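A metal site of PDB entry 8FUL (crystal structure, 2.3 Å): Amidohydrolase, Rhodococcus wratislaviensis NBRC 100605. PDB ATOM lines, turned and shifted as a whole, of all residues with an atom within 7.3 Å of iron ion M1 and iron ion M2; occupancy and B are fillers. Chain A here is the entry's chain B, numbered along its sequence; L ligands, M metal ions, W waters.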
ATOM      1  N   ALA A  24     -22.255   0.791  24.780  1.00  0.00           N
ATOM      2  CA  ALA A  24     -23.701   0.818  24.848  1.00  0.00           C
ATOM      3  C   ALA A  24     -24.278   2.222  24.809  1.00  0.00           C
ATOM      4  O   ALA A  24     -25.510   2.371  24.834  1.00  0.00           O
ATOM      5  CB  ALA A  24     -24.186   0.109  26.111  1.00  0.00           C
ATOM      6  N   ASP A  25     -23.453   3.260  24.748  1.00  0.00           N
ATOM      7  CA  ASP A  25     -24.002   4.614  24.757  1.00  0.00           C
ATOM      8  C   ASP A  25     -23.115   5.518  23.903  1.00  0.00           C
ATOM      9  O   ASP A  25     -22.099   6.017  24.387  1.00  0.00           O
ATOM     10  CB  ASP A  25     -24.143   5.160  26.175  1.00  0.00           C
ATOM     11  CG  ASP A  25     -25.093   6.344  26.234  1.00  0.00           C
ATOM     12  OD1 ASP A  25     -25.847   6.549  25.255  1.00  0.00           O
ATOM     13  OD2 ASP A  25     -25.092   7.080  27.237  1.00  0.00           O
ATOM     14  N   ILE A  26     -23.555   5.762  22.673  1.00  0.00           N
ATOM     15  CA  ILE A  26     -22.966   6.767  21.793  1.00  0.00           C
ATOM     16  C   ILE A  26     -24.039   7.798  21.472  1.00  0.00           C
ATOM     17  O   ILE A  26     -25.202   7.427  21.239  1.00  0.00           O
ATOM     18  CB  ILE A  26     -22.404   6.110  20.517  1.00  0.00           C
ATOM     19  CG1 ILE A  26     -21.427   4.979  20.901  1.00  0.00           C
ATOM     20  CG2 ILE A  26     -21.725   7.125  19.645  1.00  0.00           C
ATOM     21  CD1 ILE A  26     -20.885   4.177  19.745  1.00  0.00           C
ATOM     22  N   HIS A  27     -23.681   9.084  21.458  1.00  0.00           N
ATOM     23  CA  HIS A  27     -24.641  10.173  21.258  1.00  0.00           C
ATOM     24  C   HIS A  27     -24.337  10.952  19.988  1.00  0.00           C
ATOM     25  O   HIS A  27     -23.694  12.004  20.031  1.00  0.00           O
ATOM     26  CB  HIS A  27     -24.662  11.155  22.433  1.00  0.00           C
ATOM     27  CG  HIS A  27     -25.184  10.566  23.695  1.00  0.00           C
ATOM     28  ND1 HIS A  27     -26.344   9.827  23.747  1.00  0.00           N
ATOM     29  CD2 HIS A  27     -24.703  10.610  24.959  1.00  0.00           C
ATOM     30  CE1 HIS A  27     -26.559   9.429  24.989  1.00  0.00           C
ATOM     31  NE2 HIS A  27     -25.575   9.890  25.743  1.00  0.00           N
ATOM     32  N   ALA A  71     -21.154  20.689  28.572  1.00  0.00           N
ATOM     33  CA  ALA A  71     -20.852  19.337  29.067  1.00  0.00           C
ATOM     34  C   ALA A  71     -20.362  18.403  27.955  1.00  0.00           C
ATOM     35  O   ALA A  71     -20.454  17.170  28.073  1.00  0.00           O
ATOM     36  CB  ALA A  71     -22.063  18.724  29.777  1.00  0.00           C
ATOM     37  N   GLN A 106     -27.679   6.237  20.697  1.00  0.00           N
ATOM     38  CA  GLN A 106     -28.800   6.744  21.500  1.00  0.00           C
ATOM     39  C   GLN A 106     -28.986   8.218  21.172  1.00  0.00           C
ATOM     40  O   GLN A 106     -28.421   9.083  21.864  1.00  0.00           O
ATOM     41  CB  GLN A 106     -28.554   6.531  22.971  1.00  0.00           C
ATOM     42  CG  GLN A 106     -28.147   5.131  23.245  1.00  0.00           C
ATOM     43  CD  GLN A 106     -28.412   4.741  24.645  1.00  0.00           C
ATOM     44  OE1 GLN A 106     -28.659   5.580  25.508  1.00  0.00           O
ATOM     45  NE2 GLN A 106     -28.382   3.441  24.896  1.00  0.00           N
ATOM     46  N   LEU A 108     -30.524  11.567  21.431  1.00  0.00           N
ATOM     47  CA  LEU A 108     -31.296  12.268  22.449  1.00  0.00           C
ATOM     48  C   LEU A 108     -31.638  13.702  22.067  1.00  0.00           C
ATOM     49  O   LEU A 108     -32.009  14.480  22.942  1.00  0.00           O
ATOM     50  CB  LEU A 108     -30.550  12.300  23.781  1.00  0.00           C
ATOM     51  CG  LEU A 108     -29.901  11.085  24.458  1.00  0.00           C
ATOM     52  CD1 LEU A 108     -29.306  11.554  25.785  1.00  0.00           C
ATOM     53  CD2 LEU A 108     -30.871   9.933  24.652  1.00  0.00           C
ATOM     54  N   THR A 114     -27.552  18.858  23.978  1.00  0.00           N
ATOM     55  CA  THR A 114     -27.094  17.709  24.749  1.00  0.00           C
ATOM     56  C   THR A 114     -28.228  16.733  25.115  1.00  0.00           C
ATOM     57  O   THR A 114     -28.072  15.513  24.968  1.00  0.00           O
ATOM     58  CB  THR A 114     -26.400  18.191  26.034  1.00  0.00           C
ATOM     59  OG1 THR A 114     -25.159  18.837  25.721  1.00  0.00           O
ATOM     60  CG2 THR A 114     -26.160  17.035  27.019  1.00  0.00           C
ATOM     61  N   HIS A 211     -32.241   5.543  29.114  1.00  0.00           N
ATOM     62  CA  HIS A 211     -31.124   6.460  29.249  1.00  0.00           C
ATOM     63  C   HIS A 211     -31.488   7.636  30.155  1.00  0.00           C
ATOM     64  O   HIS A 211     -32.615   8.125  30.121  1.00  0.00           O
ATOM     65  CB  HIS A 211     -30.706   6.987  27.885  1.00  0.00           C
ATOM     66  CG  HIS A 211     -29.480   7.839  27.918  1.00  0.00           C
ATOM     67  ND1 HIS A 211     -29.496   9.162  28.319  1.00  0.00           N
ATOM     68  CD2 HIS A 211     -28.182   7.556  27.623  1.00  0.00           C
ATOM     69  CE1 HIS A 211     -28.273   9.660  28.270  1.00  0.00           C
ATOM     70  NE2 HIS A 211     -27.460   8.709  27.850  1.00  0.00           N
ATOM     71  N   LEU A 212     -30.519   8.067  30.944  1.00  0.00           N
ATOM     72  CA  LEU A 212     -30.623   9.253  31.779  1.00  0.00           C
ATOM     73  C   LEU A 212     -31.368  10.361  31.061  1.00  0.00           C
ATOM     74  O   LEU A 212     -31.123  10.614  29.877  1.00  0.00           O
ATOM     75  CB  LEU A 212     -29.209   9.715  32.166  1.00  0.00           C
ATOM     76  CG  LEU A 212     -28.824  11.070  32.742  1.00  0.00           C
ATOM     77  CD1 LEU A 212     -27.577  10.873  33.579  1.00  0.00           C
ATOM     78  CD2 LEU A 212     -28.581  12.157  31.669  1.00  0.00           C
ATOM     79  N   HIS A 233     -26.868  16.397  38.862  1.00  0.00           N
ATOM     80  CA  HIS A 233     -26.181  15.315  38.180  1.00  0.00           C
ATOM     81  C   HIS A 233     -26.092  14.071  39.058  1.00  0.00           C
ATOM     82  O   HIS A 233     -26.440  12.969  38.611  1.00  0.00           O
ATOM     83  CB  HIS A 233     -24.808  15.791  37.699  1.00  0.00           C
ATOM     84  CG  HIS A 233     -24.215  14.921  36.639  1.00  0.00           C
ATOM     85  ND1 HIS A 233     -22.996  15.184  36.052  1.00  0.00           N
ATOM     86  CD2 HIS A 233     -24.647  13.763  36.079  1.00  0.00           C
ATOM     87  CE1 HIS A 233     -22.713  14.237  35.183  1.00  0.00           C
ATOM     88  NE2 HIS A 233     -23.703  13.359  35.175  1.00  0.00           N
ATOM     89  N   VAL A 264     -29.210   2.911  31.436  1.00  0.00           N
ATOM     90  CA  VAL A 264     -28.049   3.522  30.789  1.00  0.00           C
ATOM     91  C   VAL A 264     -27.721   4.859  31.456  1.00  0.00           C
ATOM     92  O   VAL A 264     -28.572   5.763  31.486  1.00  0.00           O
ATOM     93  CB  VAL A 264     -28.251   3.700  29.277  1.00  0.00           C
ATOM     94  CG1 VAL A 264     -27.035   4.356  28.690  1.00  0.00           C
ATOM     95  CG2 VAL A 264     -28.487   2.354  28.614  1.00  0.00           C
ATOM     96  N   GLU A 265     -26.491   4.981  31.946  1.00  0.00           N
ATOM     97  CA  GLU A 265     -25.940   6.222  32.489  1.00  0.00           C
ATOM     98  C   GLU A 265     -26.592   6.593  33.826  1.00  0.00           C
ATOM     99  O   GLU A 265     -26.830   7.756  34.117  1.00  0.00           O
ATOM    100  CB  GLU A 265     -26.019   7.385  31.478  1.00  0.00           C
ATOM    101  CG  GLU A 265     -25.146   8.553  31.857  1.00  0.00           C
ATOM    102  CD  GLU A 265     -24.828   9.459  30.718  1.00  0.00           C
ATOM    103  OE1 GLU A 265     -25.089   9.065  29.569  1.00  0.00           O
ATOM    104  OE2 GLU A 265     -24.292  10.569  30.974  1.00  0.00           O
ATOM    105  N   SER A 307     -25.304  -0.123  32.106  1.00  0.00           N
ATOM    106  CA  SER A 307     -24.061   0.342  31.514  1.00  0.00           C
ATOM    107  C   SER A 307     -23.218   1.040  32.586  1.00  0.00           C
ATOM    108  O   SER A 307     -23.690   1.327  33.680  1.00  0.00           O
ATOM    109  CB  SER A 307     -24.340   1.252  30.319  1.00  0.00           C
ATOM    110  OG  SER A 307     -24.697   2.555  30.741  1.00  0.00           O
ATOM    111  N   GLN A 309     -20.690   3.920  32.245  1.00  0.00           N
ATOM    112  CA  GLN A 309     -20.450   5.341  32.288  1.00  0.00           C
ATOM    113  C   GLN A 309     -21.528   6.046  33.114  1.00  0.00           C
ATOM    114  O   GLN A 309     -22.715   5.715  33.005  1.00  0.00           O
ATOM    115  CB  GLN A 309     -20.412   5.906  30.856  1.00  0.00           C
ATOM    116  CG  GLN A 309     -19.789   7.317  30.726  1.00  0.00           C
ATOM    117  CD  GLN A 309     -20.795   8.411  31.003  1.00  0.00           C
ATOM    118  OE1 GLN A 309     -21.976   8.130  31.121  1.00  0.00           O
ATOM    119  NE2 GLN A 309     -20.348   9.643  31.044  1.00  0.00           N
ATOM    120  N   PRO A 310     -21.157   7.010  33.980  1.00  0.00           N
ATOM    121  CA  PRO A 310     -19.764   7.331  34.335  1.00  0.00           C
ATOM    122  C   PRO A 310     -19.268   6.373  35.417  1.00  0.00           C
ATOM    123  O   PRO A 310     -19.945   6.236  36.431  1.00  0.00           O
ATOM    124  CB  PRO A 310     -19.853   8.758  34.866  1.00  0.00           C
ATOM    125  CG  PRO A 310     -21.229   8.889  35.407  1.00  0.00           C
ATOM    126  CD  PRO A 310     -22.122   7.916  34.633  1.00  0.00           C
ATOM    127  N   ALA A 335     -19.741   1.285  28.478  1.00  0.00           N
ATOM    128  CA  ALA A 335     -20.144   2.391  27.612  1.00  0.00           C
ATOM    129  C   ALA A 335     -19.170   3.546  27.757  1.00  0.00           C
ATOM    130  O   ALA A 335     -18.571   3.745  28.826  1.00  0.00           O
ATOM    131  CB  ALA A 335     -21.586   2.841  27.911  1.00  0.00           C
ATOM    132  N   THR A 336     -19.005   4.321  26.687  1.00  0.00           N
ATOM    133  CA  THR A 336     -18.157   5.498  26.709  1.00  0.00           C
ATOM    134  C   THR A 336     -18.919   6.799  26.952  1.00  0.00           C
ATOM    135  O   THR A 336     -18.354   7.726  27.513  1.00  0.00           O
ATOM    136  CB  THR A 336     -17.397   5.666  25.390  1.00  0.00           C
ATOM    137  OG1 THR A 336     -18.305   5.953  24.324  1.00  0.00           O
ATOM    138  CG2 THR A 336     -16.545   4.439  25.059  1.00  0.00           C
ATOM    139  N   ASP A 337     -20.149   6.895  26.461  1.00  0.00           N
ATOM    140  CA  ASP A 337     -20.887   8.155  26.456  1.00  0.00           C
ATOM    141  C   ASP A 337     -20.211   9.186  25.558  1.00  0.00           C
ATOM    142  O   ASP A 337     -20.201  10.386  25.837  1.00  0.00           O
ATOM    143  CB  ASP A 337     -21.040   8.708  27.876  1.00  0.00           C
ATOM    144  CG  ASP A 337     -22.153   9.695  27.978  1.00  0.00           C
ATOM    145  OD1 ASP A 337     -23.094   9.572  27.178  1.00  0.00           O
ATOM    146  OD2 ASP A 337     -22.075  10.586  28.850  1.00  0.00           O
ATOM    147  N   TYR A 338     -19.645   8.736  24.463  1.00  0.00           N
ATOM    148  CA  TYR A 338     -19.100   9.689  23.511  1.00  0.00           C
ATOM    149  C   TYR A 338     -20.222  10.544  22.946  1.00  0.00           C
ATOM    150  O   TYR A 338     -21.243  10.003  22.503  1.00  0.00           O
ATOM    151  CB  TYR A 338     -18.344   8.956  22.404  1.00  0.00           C
ATOM    152  CG  TYR A 338     -17.778   9.899  21.377  1.00  0.00           C
ATOM    153  CD1 TYR A 338     -16.546  10.497  21.567  1.00  0.00           C
ATOM    154  CD2 TYR A 338     -18.499  10.211  20.226  1.00  0.00           C
ATOM    155  CE1 TYR A 338     -16.029  11.369  20.638  1.00  0.00           C
ATOM    156  CE2 TYR A 338     -18.004  11.092  19.290  1.00  0.00           C
ATOM    157  CZ  TYR A 338     -16.768  11.666  19.495  1.00  0.00           C
ATOM    158  OH  TYR A 338     -16.262  12.537  18.566  1.00  0.00           O
ATOM    159  N   PRO A 339     -20.085  11.889  22.903  1.00  0.00           N
ATOM    160  CA  PRO A 339     -18.912  12.706  23.229  1.00  0.00           C
ATOM    161  C   PRO A 339     -19.038  13.572  24.484  1.00  0.00           C
ATOM    162  O   PRO A 339     -18.481  14.667  24.509  1.00  0.00           O
ATOM    163  CB  PRO A 339     -18.805  13.603  22.005  1.00  0.00           C
ATOM    164  CG  PRO A 339     -20.269  13.954  21.748  1.00  0.00           C
ATOM    165  CD  PRO A 339     -21.084  12.714  22.182  1.00  0.00           C
ATOM    166  N   HIS A 340     -19.763  13.125  25.510  1.00  0.00           N
ATOM    167  CA  HIS A 340     -19.990  13.981  26.664  1.00  0.00           C
ATOM    168  C   HIS A 340     -18.690  14.136  27.488  1.00  0.00           C
ATOM    169  O   HIS A 340     -17.714  13.409  27.308  1.00  0.00           O
ATOM    170  CB  HIS A 340     -21.125  13.417  27.516  1.00  0.00           C
ATOM    171  CG  HIS A 340     -22.481  13.541  26.883  1.00  0.00           C
ATOM    172  ND1 HIS A 340     -23.619  13.052  27.465  1.00  0.00           N
ATOM    173  CD2 HIS A 340     -22.864  14.109  25.716  1.00  0.00           C
ATOM    174  CE1 HIS A 340     -24.660  13.295  26.682  1.00  0.00           C
ATOM    175  NE2 HIS A 340     -24.225  13.940  25.611  1.00  0.00           N
ATOM    176  N   PHE A 341     -18.713  15.105  28.413  1.00  0.00           N
ATOM    177  CA  PHE A 341     -17.475  15.546  29.049  1.00  0.00           C
ATOM    178  C   PHE A 341     -16.916  14.487  29.981  1.00  0.00           C
ATOM    179  O   PHE A 341     -15.691  14.398  30.134  1.00  0.00           O
ATOM    180  CB  PHE A 341     -17.688  16.858  29.815  1.00  0.00           C
ATOM    181  CG  PHE A 341     -18.215  16.687  31.236  1.00  0.00           C
ATOM    182  CD1 PHE A 341     -19.584  16.681  31.488  1.00  0.00           C
ATOM    183  CD2 PHE A 341     -17.330  16.573  32.303  1.00  0.00           C
ATOM    184  CE1 PHE A 341     -20.068  16.553  32.794  1.00  0.00           C
ATOM    185  CE2 PHE A 341     -17.812  16.433  33.616  1.00  0.00           C
ATOM    186  CZ  PHE A 341     -19.182  16.429  33.858  1.00  0.00           C
ATOM    187  N   ASP A 342     -17.771  13.709  30.627  1.00  0.00           N
ATOM    188  CA  ASP A 342     -17.331  12.628  31.498  1.00  0.00           C
ATOM    189  C   ASP A 342     -17.197  11.300  30.752  1.00  0.00           C
ATOM    190  O   ASP A 342     -17.386  10.221  31.341  1.00  0.00           O
ATOM    191  CB  ASP A 342     -18.262  12.513  32.713  1.00  0.00           C
ATOM    192  CG  ASP A 342     -19.729  12.365  32.330  1.00  0.00           C
ATOM    193  OD1 ASP A 342     -20.098  12.760  31.204  1.00  0.00           O
ATOM    194  OD2 ASP A 342     -20.516  11.837  33.144  1.00  0.00           O
ATOM    195  N   PHE A 343     -16.887  11.372  29.450  1.00  0.00           N
ATOM    196  CA  PHE A 343     -16.517  10.229  28.624  1.00  0.00           C
ATOM    197  C   PHE A 343     -15.581   9.278  29.360  1.00  0.00           C
ATOM    198  O   PHE A 343     -14.673   9.701  30.057  1.00  0.00           O
ATOM    199  CB  PHE A 343     -15.856  10.759  27.342  1.00  0.00           C
ATOM    200  CG  PHE A 343     -15.049   9.753  26.581  1.00  0.00           C
ATOM    201  CD1 PHE A 343     -15.612   9.071  25.511  1.00  0.00           C
ATOM    202  CD2 PHE A 343     -13.713   9.529  26.884  1.00  0.00           C
ATOM    203  CE1 PHE A 343     -14.858   8.154  24.783  1.00  0.00           C
ATOM    204  CE2 PHE A 343     -12.959   8.618  26.177  1.00  0.00           C
ATOM    205  CZ  PHE A 343     -13.530   7.920  25.124  1.00  0.00           C
HETATM  206  C1  LIG L   1     -23.253  13.941  31.725  1.00  0.00           C
HETATM  207  O1  LIG L   1     -22.590  13.153  30.753  1.00  0.00           O
HETATM  208  C2  LIG L   1     -24.364  14.776  31.031  1.00  0.00           C
HETATM  209  O2  LIG L   1     -23.964  15.221  29.782  1.00  0.00           O
HETATM  210  C3  LIG L   1     -25.577  13.821  30.871  1.00  0.00           C
HETATM  211  O3  LIG L   1     -26.365  14.328  29.779  1.00  0.00           O
HETATM  212 FE    FE M   1     -23.811  12.019  29.339  1.00  0.00          FE
HETATM  213 FE    FE M   2     -25.230   8.909  27.535  1.00  0.00          FE
HETATM  214  O   HOH W   1     -25.450  10.862  28.307  1.00  0.00           O
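Iron ion M2 is bound by OD2 of Asp 25 (1.9 Å), OE1 of Glu 265 (2.0 Å), NE2 of His 27 (2.1 Å), water W1 (2.1 Å), NE2 of His 211 (2.3 Å) and OD1 of Asp 337 (2.3 Å). Iron ion M2 has six donor atoms within binding distance.
The nearest printed residue that does not touch iron ion M1 is Asp 342 (4.2 Å).
OE1 of Gln 106 lies close to OD1 of Asp 25. ND1 of His 27 lies within hydrogen-bond range of O of Gln 106, at 2.9 Å. The side-chain hydroxyl (OG) of Ser 307 is in hydrogen-bond range of the backbone NH (N) of Glu 265 (3.2 Å). N of His 27 sits at hydrogen-bond distance from O of Tyr 338 (2.8 Å). The side-chain amide oxygen of Gln 309 sits close to the side-chain carboxylate of Glu 265, 3.4 Å away. OD2 of Asp 337 sits close to NE2 of Gln 309.
A ring nitrogen (ND1) of His 340 is bound to iron ion M1 (2.1 Å). O1 of the ligand binds iron ion M1, at 2.2 Å. Iron ion M1 is bound by the side-chain carboxylate (OE2) of Glu 265. Water W1 is bound to iron ion M1. OD2 of Asp 337 binds iron ion M1, 2.3 Å away. Iron ion M1 has five donor atoms within binding distance.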
